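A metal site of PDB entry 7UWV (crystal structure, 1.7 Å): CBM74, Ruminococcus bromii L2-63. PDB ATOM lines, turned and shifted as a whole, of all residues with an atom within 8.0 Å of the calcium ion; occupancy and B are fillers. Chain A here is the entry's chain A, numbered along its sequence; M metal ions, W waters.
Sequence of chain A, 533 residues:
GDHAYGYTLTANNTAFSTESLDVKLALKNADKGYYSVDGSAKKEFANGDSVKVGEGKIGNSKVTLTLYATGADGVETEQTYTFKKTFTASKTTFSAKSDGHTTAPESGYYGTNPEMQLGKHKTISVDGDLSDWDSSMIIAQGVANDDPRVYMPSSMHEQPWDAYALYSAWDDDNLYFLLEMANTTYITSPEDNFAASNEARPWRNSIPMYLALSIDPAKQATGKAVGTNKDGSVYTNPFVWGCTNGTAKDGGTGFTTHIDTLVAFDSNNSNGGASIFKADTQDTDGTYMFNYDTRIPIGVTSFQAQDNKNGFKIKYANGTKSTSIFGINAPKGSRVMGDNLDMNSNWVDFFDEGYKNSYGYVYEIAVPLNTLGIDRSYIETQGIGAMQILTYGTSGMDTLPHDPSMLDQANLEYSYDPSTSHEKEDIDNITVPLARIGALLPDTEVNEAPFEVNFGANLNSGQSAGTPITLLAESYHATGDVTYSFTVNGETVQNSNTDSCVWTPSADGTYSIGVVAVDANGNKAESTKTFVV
The calcium ion is bound by OD1 of Asp 162, O of Ala 163, OD1 of Asp 146, OD2 of Asp 398, O of Val 143 and water W1.
The side-chain carboxylate (OD2) of Asp 146 sits at hydrogen-bond distance from the side-chain hydroxyl (OH) of Tyr 110, at 2.5 Å.
The backbone NH of Ala 182 lies within hydrogen-bond range of the backbone carbonyl oxygen of Asp 162 (2.9 Å).
The backbone NH (N) of Leu 390 is in hydrogen-bond range of the backbone carbonyl oxygen (O) of Asp 398 (2.9 Å).
N of Asn 145 lies within hydrogen-bond range of OD2 of Asp 162.
Five residues have an atom within 4 Å of the calcium ion: Val 143, Asp 146, Asp 162, Ala 163 and Asp 398.
Water W1 lies within hydrogen-bond range of OD2 of Asp 146 (2.7 Å), OD1 of Asp 398 (3.0 Å) and N of Val 143 (3.4 Å).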
ATOM      1  N   TYR A 110     -29.919  19.859 -20.100  1.00  0.00           N
ATOM      2  CA  TYR A 110     -29.616  21.229 -20.567  1.00  0.00           C
ATOM      3  C   TYR A 110     -30.578  21.604 -21.694  1.00  0.00           C
ATOM      4  O   TYR A 110     -31.040  20.714 -22.419  1.00  0.00           O
ATOM      5  CB  TYR A 110     -28.181  21.348 -21.071  1.00  0.00           C
ATOM      6  CG  TYR A 110     -27.125  21.065 -20.038  1.00  0.00           C
ATOM      7  CD1 TYR A 110     -26.658  22.054 -19.188  1.00  0.00           C
ATOM      8  CD2 TYR A 110     -26.583  19.805 -19.905  1.00  0.00           C
ATOM      9  CE1 TYR A 110     -25.676  21.810 -18.248  1.00  0.00           C
ATOM     10  CE2 TYR A 110     -25.601  19.525 -18.964  1.00  0.00           C
ATOM     11  CZ  TYR A 110     -25.149  20.530 -18.132  1.00  0.00           C
ATOM     12  OH  TYR A 110     -24.154  20.251 -17.226  1.00  0.00           O
ATOM     13  N   GLN A 141     -31.652  26.703 -19.672  1.00  0.00           N
ATOM     14  CA  GLN A 141     -31.793  25.715 -18.581  1.00  0.00           C
ATOM     15  C   GLN A 141     -30.465  24.978 -18.405  1.00  0.00           C
ATOM     16  O   GLN A 141     -29.988  24.342 -19.377  1.00  0.00           O
ATOM     17  CB  GLN A 141     -32.950  24.764 -18.887  1.00  0.00           C
ATOM     18  CG  GLN A 141     -33.258  23.762 -17.774  1.00  0.00           C
ATOM     19  CD  GLN A 141     -33.638  24.439 -16.476  1.00  0.00           C
ATOM     20  OE1 GLN A 141     -34.673  25.076 -16.360  1.00  0.00           O
ATOM     21  NE2 GLN A 141     -32.778  24.316 -15.473  1.00  0.00           N
ATOM     22  N   GLY A 142     -29.865  25.099 -17.223  1.00  0.00           N
ATOM     23  CA  GLY A 142     -28.683  24.332 -16.813  1.00  0.00           C
ATOM     24  C   GLY A 142     -29.067  23.201 -15.892  1.00  0.00           C
ATOM     25  O   GLY A 142     -30.255  22.798 -15.825  1.00  0.00           O
ATOM     26  N   VAL A 143     -28.080  22.686 -15.156  1.00  0.00           N
ATOM     27  CA  VAL A 143     -28.302  21.606 -14.160  1.00  0.00           C
ATOM     28  C   VAL A 143     -27.576  22.003 -12.880  1.00  0.00           C
ATOM     29  O   VAL A 143     -26.691  22.873 -12.938  1.00  0.00           O
ATOM     30  CB  VAL A 143     -27.890  20.218 -14.673  1.00  0.00           C
ATOM     31  CG1 VAL A 143     -28.434  19.946 -16.061  1.00  0.00           C
ATOM     32  CG2 VAL A 143     -26.389  20.025 -14.644  1.00  0.00           C
ATOM     33  N   ALA A 144     -27.971  21.373 -11.789  1.00  0.00           N
ATOM     34  CA  ALA A 144     -27.311  21.504 -10.478  1.00  0.00           C
ATOM     35  C   ALA A 144     -26.151  20.518 -10.407  1.00  0.00           C
ATOM     36  O   ALA A 144     -26.219  19.452 -11.029  1.00  0.00           O
ATOM     37  CB  ALA A 144     -28.316  21.269  -9.378  1.00  0.00           C
ATOM     38  N   ASN A 145     -25.092  20.901  -9.681  1.00  0.00           N
ATOM     39  CA  ASN A 145     -23.967  20.022  -9.278  1.00  0.00           C
ATOM     40  C   ASN A 145     -23.133  19.614 -10.504  1.00  0.00           C
ATOM     41  O   ASN A 145     -22.626  18.459 -10.520  1.00  0.00           O
ATOM     42  CB  ASN A 145     -24.480  18.820  -8.470  1.00  0.00           C
ATOM     43  CG  ASN A 145     -23.417  18.248  -7.552  1.00  0.00           C
ATOM     44  OD1 ASN A 145     -22.592  18.983  -7.004  1.00  0.00           O
ATOM     45  ND2 ASN A 145     -23.417  16.935  -7.381  1.00  0.00           N
ATOM     46  N   ASP A 146     -22.931  20.532 -11.459  1.00  0.00           N
ATOM     47  CA  ASP A 146     -22.012  20.357 -12.612  1.00  0.00           C
ATOM     48  C   ASP A 146     -20.947  21.463 -12.601  1.00  0.00           C
ATOM     49  O   ASP A 146     -20.303  21.651 -13.637  1.00  0.00           O
ATOM     50  CB  ASP A 146     -22.753  20.381 -13.947  1.00  0.00           C
ATOM     51  CG  ASP A 146     -23.392  21.719 -14.233  1.00  0.00           C
ATOM     52  OD1 ASP A 146     -23.561  22.503 -13.275  1.00  0.00           O
ATOM     53  OD2 ASP A 146     -23.725  21.972 -15.422  1.00  0.00           O
ATOM     54  N   ASP A 147     -20.776  22.185 -11.486  1.00  0.00           N
ATOM     55  CA  ASP A 147     -19.699  23.189 -11.348  1.00  0.00           C
ATOM     56  C   ASP A 147     -18.374  22.457 -11.164  1.00  0.00           C
ATOM     57  O   ASP A 147     -18.352  21.325 -10.676  1.00  0.00           O
ATOM     58  CB  ASP A 147     -20.006  24.223 -10.258  1.00  0.00           C
ATOM     59  CG  ASP A 147     -20.340  23.656  -8.895  1.00  0.00           C
ATOM     60  OD1 ASP A 147     -21.174  22.723  -8.826  1.00  0.00           O
ATOM     61  OD2 ASP A 147     -19.759  24.151  -7.904  1.00  0.00           O
ATOM     62  N   PRO A 148     -17.232  23.034 -11.597  1.00  0.00           N
ATOM     63  CA  PRO A 148     -15.972  22.296 -11.711  1.00  0.00           C
ATOM     64  C   PRO A 148     -15.459  21.563 -10.453  1.00  0.00           C
ATOM     65  O   PRO A 148     -14.823  20.525 -10.605  1.00  0.00           O
ATOM     66  CB  PRO A 148     -14.979  23.390 -12.125  1.00  0.00           C
ATOM     67  CG  PRO A 148     -15.846  24.336 -12.938  1.00  0.00           C
ATOM     68  CD  PRO A 148     -17.114  24.409 -12.111  1.00  0.00           C
ATOM     69  N   TRP A 161     -20.103  27.514  -7.511  1.00  0.00           N
ATOM     70  CA  TRP A 161     -20.487  28.501  -8.554  1.00  0.00           C
ATOM     71  C   TRP A 161     -21.405  27.767  -9.531  1.00  0.00           C
ATOM     72  O   TRP A 161     -20.952  27.431 -10.643  1.00  0.00           O
ATOM     73  CB  TRP A 161     -19.246  29.156  -9.157  1.00  0.00           C
ATOM     74  CG  TRP A 161     -18.582  29.965  -8.097  1.00  0.00           C
ATOM     75  CD1 TRP A 161     -17.583  29.575  -7.252  1.00  0.00           C
ATOM     76  CD2 TRP A 161     -19.018  31.258  -7.628  1.00  0.00           C
ATOM     77  NE1 TRP A 161     -17.321  30.552  -6.331  1.00  0.00           N
ATOM     78  CE2 TRP A 161     -18.177  31.603  -6.550  1.00  0.00           C
ATOM     79  CE3 TRP A 161     -20.001  32.161  -8.046  1.00  0.00           C
ATOM     80  CZ2 TRP A 161     -18.315  32.818  -5.866  1.00  0.00           C
ATOM     81  CZ3 TRP A 161     -20.122  33.352  -7.377  1.00  0.00           C
ATOM     82  CH2 TRP A 161     -19.300  33.674  -6.303  1.00  0.00           C
ATOM     83  N   ASP A 162     -22.626  27.490  -9.081  1.00  0.00           N
ATOM     84  CA  ASP A 162     -23.526  26.507  -9.726  1.00  0.00           C
ATOM     85  C   ASP A 162     -24.746  27.228 -10.297  1.00  0.00           C
ATOM     86  O   ASP A 162     -25.786  27.306  -9.606  1.00  0.00           O
ATOM     87  CB  ASP A 162     -23.908  25.395  -8.754  1.00  0.00           C
ATOM     88  CG  ASP A 162     -24.697  24.270  -9.400  1.00  0.00           C
ATOM     89  OD1 ASP A 162     -24.751  24.232 -10.666  1.00  0.00           O
ATOM     90  OD2 ASP A 162     -25.219  23.412  -8.657  1.00  0.00           O
ATOM     91  N   ALA A 163     -24.650  27.672 -11.548  1.00  0.00           N
ATOM     92  CA  ALA A 163     -25.764  28.278 -12.292  1.00  0.00           C
ATOM     93  C   ALA A 163     -26.822  27.208 -12.568  1.00  0.00           C
ATOM     94  O   ALA A 163     -26.440  26.083 -12.957  1.00  0.00           O
ATOM     95  CB  ALA A 163     -25.270  28.903 -13.572  1.00  0.00           C
ATOM     96  N   TYR A 164     -28.106  27.546 -12.414  1.00  0.00           N
ATOM     97  CA  TYR A 164     -29.210  26.584 -12.628  1.00  0.00           C
ATOM     98  C   TYR A 164     -30.093  27.020 -13.805  1.00  0.00           C
ATOM     99  O   TYR A 164     -30.323  26.187 -14.713  1.00  0.00           O
ATOM    100  CB  TYR A 164     -30.058  26.333 -11.370  1.00  0.00           C
ATOM    101  CG  TYR A 164     -30.987  25.176 -11.614  1.00  0.00           C
ATOM    102  CD1 TYR A 164     -30.489  23.890 -11.746  1.00  0.00           C
ATOM    103  CD2 TYR A 164     -32.339  25.374 -11.858  1.00  0.00           C
ATOM    104  CE1 TYR A 164     -31.311  22.817 -12.033  1.00  0.00           C
ATOM    105  CE2 TYR A 164     -33.177  24.309 -12.157  1.00  0.00           C
ATOM    106  CZ  TYR A 164     -32.661  23.031 -12.251  1.00  0.00           C
ATOM    107  OH  TYR A 164     -33.456  21.978 -12.555  1.00  0.00           O
ATOM    108  N   ALA A 165     -30.604  28.244 -13.813  1.00  0.00           N
ATOM    109  CA  ALA A 165     -31.487  28.722 -14.904  1.00  0.00           C
ATOM    110  C   ALA A 165     -31.407  30.240 -15.048  1.00  0.00           C
ATOM    111  O   ALA A 165     -31.147  30.945 -14.066  1.00  0.00           O
ATOM    112  CB  ALA A 165     -32.910  28.251 -14.674  1.00  0.00           C
ATOM    113  N   GLU A 180     -30.990  31.935 -11.335  1.00  0.00           N
ATOM    114  CA  GLU A 180     -31.028  30.963 -10.206  1.00  0.00           C
ATOM    115  C   GLU A 180     -29.672  30.275 -10.116  1.00  0.00           C
ATOM    116  O   GLU A 180     -29.176  29.784 -11.156  1.00  0.00           O
ATOM    117  CB  GLU A 180     -32.073  29.872 -10.398  1.00  0.00           C
ATOM    118  CG  GLU A 180     -33.498  30.294 -10.151  1.00  0.00           C
ATOM    119  CD  GLU A 180     -34.426  29.092 -10.274  1.00  0.00           C
ATOM    120  OE1 GLU A 180     -34.636  28.633 -11.420  1.00  0.00           O
ATOM    121  OE2 GLU A 180     -34.863  28.575  -9.226  1.00  0.00           O
ATOM    122  N   MET A 181     -29.108  30.228  -8.908  1.00  0.00           N
ATOM    123  CA  MET A 181     -27.924  29.423  -8.559  1.00  0.00           C
ATOM    124  C   MET A 181     -28.341  28.398  -7.495  1.00  0.00           C
ATOM    125  O   MET A 181     -29.158  28.743  -6.613  1.00  0.00           O
ATOM    126  CB  MET A 181     -26.784  30.303  -8.045  1.00  0.00           C
ATOM    127  CG  MET A 181     -26.264  31.248  -9.092  1.00  0.00           C
ATOM    128  SD  MET A 181     -25.127  32.494  -8.451  1.00  0.00           S
ATOM    129  CE  MET A 181     -23.867  31.473  -7.696  1.00  0.00           C
ATOM    130  N   ALA A 182     -27.832  27.174  -7.602  1.00  0.00           N
ATOM    131  CA  ALA A 182     -28.177  26.074  -6.676  1.00  0.00           C
ATOM    132  C   ALA A 182     -27.008  25.824  -5.726  1.00  0.00           C
ATOM    133  O   ALA A 182     -25.863  26.223  -6.061  1.00  0.00           O
ATOM    134  CB  ALA A 182     -28.537  24.826  -7.447  1.00  0.00           C
ATOM    135  N   PHE A 326     -32.819  19.603 -10.965  1.00  0.00           N
ATOM    136  CA  PHE A 326     -32.238  18.381 -11.582  1.00  0.00           C
ATOM    137  C   PHE A 326     -30.712  18.467 -11.558  1.00  0.00           C
ATOM    138  O   PHE A 326     -30.132  19.492 -11.938  1.00  0.00           O
ATOM    139  CB  PHE A 326     -32.758  18.207 -13.016  1.00  0.00           C
ATOM    140  CG  PHE A 326     -34.244  17.974 -13.113  1.00  0.00           C
ATOM    141  CD1 PHE A 326     -34.817  16.820 -12.591  1.00  0.00           C
ATOM    142  CD2 PHE A 326     -35.074  18.876 -13.754  1.00  0.00           C
ATOM    143  CE1 PHE A 326     -36.170  16.588 -12.703  1.00  0.00           C
ATOM    144  CE2 PHE A 326     -36.439  18.649 -13.862  1.00  0.00           C
ATOM    145  CZ  PHE A 326     -36.979  17.499 -13.343  1.00  0.00           C
ATOM    146  N   LEU A 390     -20.541  32.721 -14.803  1.00  0.00           N
ATOM    147  CA  LEU A 390     -20.010  32.754 -13.420  1.00  0.00           C
ATOM    148  C   LEU A 390     -18.516  32.486 -13.455  1.00  0.00           C
ATOM    149  O   LEU A 390     -18.054  31.711 -14.312  1.00  0.00           O
ATOM    150  CB  LEU A 390     -20.701  31.685 -12.568  1.00  0.00           C
ATOM    151  CG  LEU A 390     -22.211  31.844 -12.387  1.00  0.00           C
ATOM    152  CD1 LEU A 390     -22.717  30.764 -11.458  1.00  0.00           C
ATOM    153  CD2 LEU A 390     -22.559  33.225 -11.845  1.00  0.00           C
ATOM    154  N   MET A 397     -16.545  29.321 -14.665  1.00  0.00           N
ATOM    155  CA  MET A 397     -16.822  28.090 -13.890  1.00  0.00           C
ATOM    156  C   MET A 397     -18.124  27.444 -14.384  1.00  0.00           C
ATOM    157  O   MET A 397     -18.187  26.199 -14.372  1.00  0.00           O
ATOM    158  CB  MET A 397     -16.953  28.413 -12.395  1.00  0.00           C
ATOM    159  CG  MET A 397     -15.680  29.012 -11.815  1.00  0.00           C
ATOM    160  SD  MET A 397     -14.399  27.752 -11.611  1.00  0.00           S
ATOM    161  CE  MET A 397     -14.850  27.058 -10.026  1.00  0.00           C
ATOM    162  N   ASP A 398     -19.130  28.235 -14.759  1.00  0.00           N
ATOM    163  CA  ASP A 398     -20.453  27.730 -15.205  1.00  0.00           C
ATOM    164  C   ASP A 398     -21.063  28.817 -16.096  1.00  0.00           C
ATOM    165  O   ASP A 398     -20.777  29.993 -15.864  1.00  0.00           O
ATOM    166  CB  ASP A 398     -21.347  27.350 -14.016  1.00  0.00           C
ATOM    167  CG  ASP A 398     -22.523  26.422 -14.331  1.00  0.00           C
ATOM    168  OD1 ASP A 398     -22.810  26.224 -15.521  1.00  0.00           O
ATOM    169  OD2 ASP A 398     -23.178  25.934 -13.359  1.00  0.00           O
ATOM    170  N   THR A 399     -21.840  28.437 -17.114  1.00  0.00           N
ATOM    171  CA  THR A 399     -22.508  29.382 -18.041  1.00  0.00           C
ATOM    172  C   THR A 399     -23.934  28.906 -18.318  1.00  0.00           C
ATOM    173  O   THR A 399     -24.188  27.707 -18.155  1.00  0.00           O
ATOM    174  CB  THR A 399     -21.731  29.536 -19.360  1.00  0.00           C
ATOM    175  OG1 THR A 399     -21.661  28.288 -20.060  1.00  0.00           O
ATOM    176  CG2 THR A 399     -20.317  30.036 -19.143  1.00  0.00           C
ATOM    177  N   LEU A 400     -24.812  29.829 -18.673  1.00  0.00           N
ATOM    178  CA  LEU A 400     -26.188  29.530 -19.167  1.00  0.00           C
ATOM    179  C   LEU A 400     -26.390  30.325 -20.442  1.00  0.00           C
ATOM    180  O   LEU A 400     -26.407  31.562 -20.377  1.00  0.00           O
ATOM    181  CB  LEU A 400     -27.208  29.930 -18.106  1.00  0.00           C
ATOM    182  CG  LEU A 400     -27.144  29.182 -16.776  1.00  0.00           C
ATOM    183  CD1 LEU A 400     -28.036  29.853 -15.740  1.00  0.00           C
ATOM    184  CD2 LEU A 400     -27.538  27.731 -16.948  1.00  0.00           C
ATOM    185  N   HIS A 402     -25.111  26.353 -21.031  1.00  0.00           N
ATOM    186  CA  HIS A 402     -23.877  25.643 -20.590  1.00  0.00           C
ATOM    187  C   HIS A 402     -22.956  25.394 -21.805  1.00  0.00           C
ATOM    188  O   HIS A 402     -23.436  25.040 -22.883  1.00  0.00           O
ATOM    189  CB  HIS A 402     -24.208  24.361 -19.838  1.00  0.00           C
ATOM    190  CG  HIS A 402     -23.020  23.821 -19.099  1.00  0.00           C
ATOM    191  ND1 HIS A 402     -22.276  22.752 -19.558  1.00  0.00           N
ATOM    192  CD2 HIS A 402     -22.421  24.243 -17.973  1.00  0.00           C
ATOM    193  CE1 HIS A 402     -21.289  22.522 -18.727  1.00  0.00           C
ATOM    194  NE2 HIS A 402     -21.354  23.434 -17.742  1.00  0.00           N
HETATM  195 CA    CA M   1     -24.878  24.388 -12.945  1.00  0.00          CA
HETATM  196  O   HOH W   1     -25.041  24.280 -15.372  1.00  0.00           O
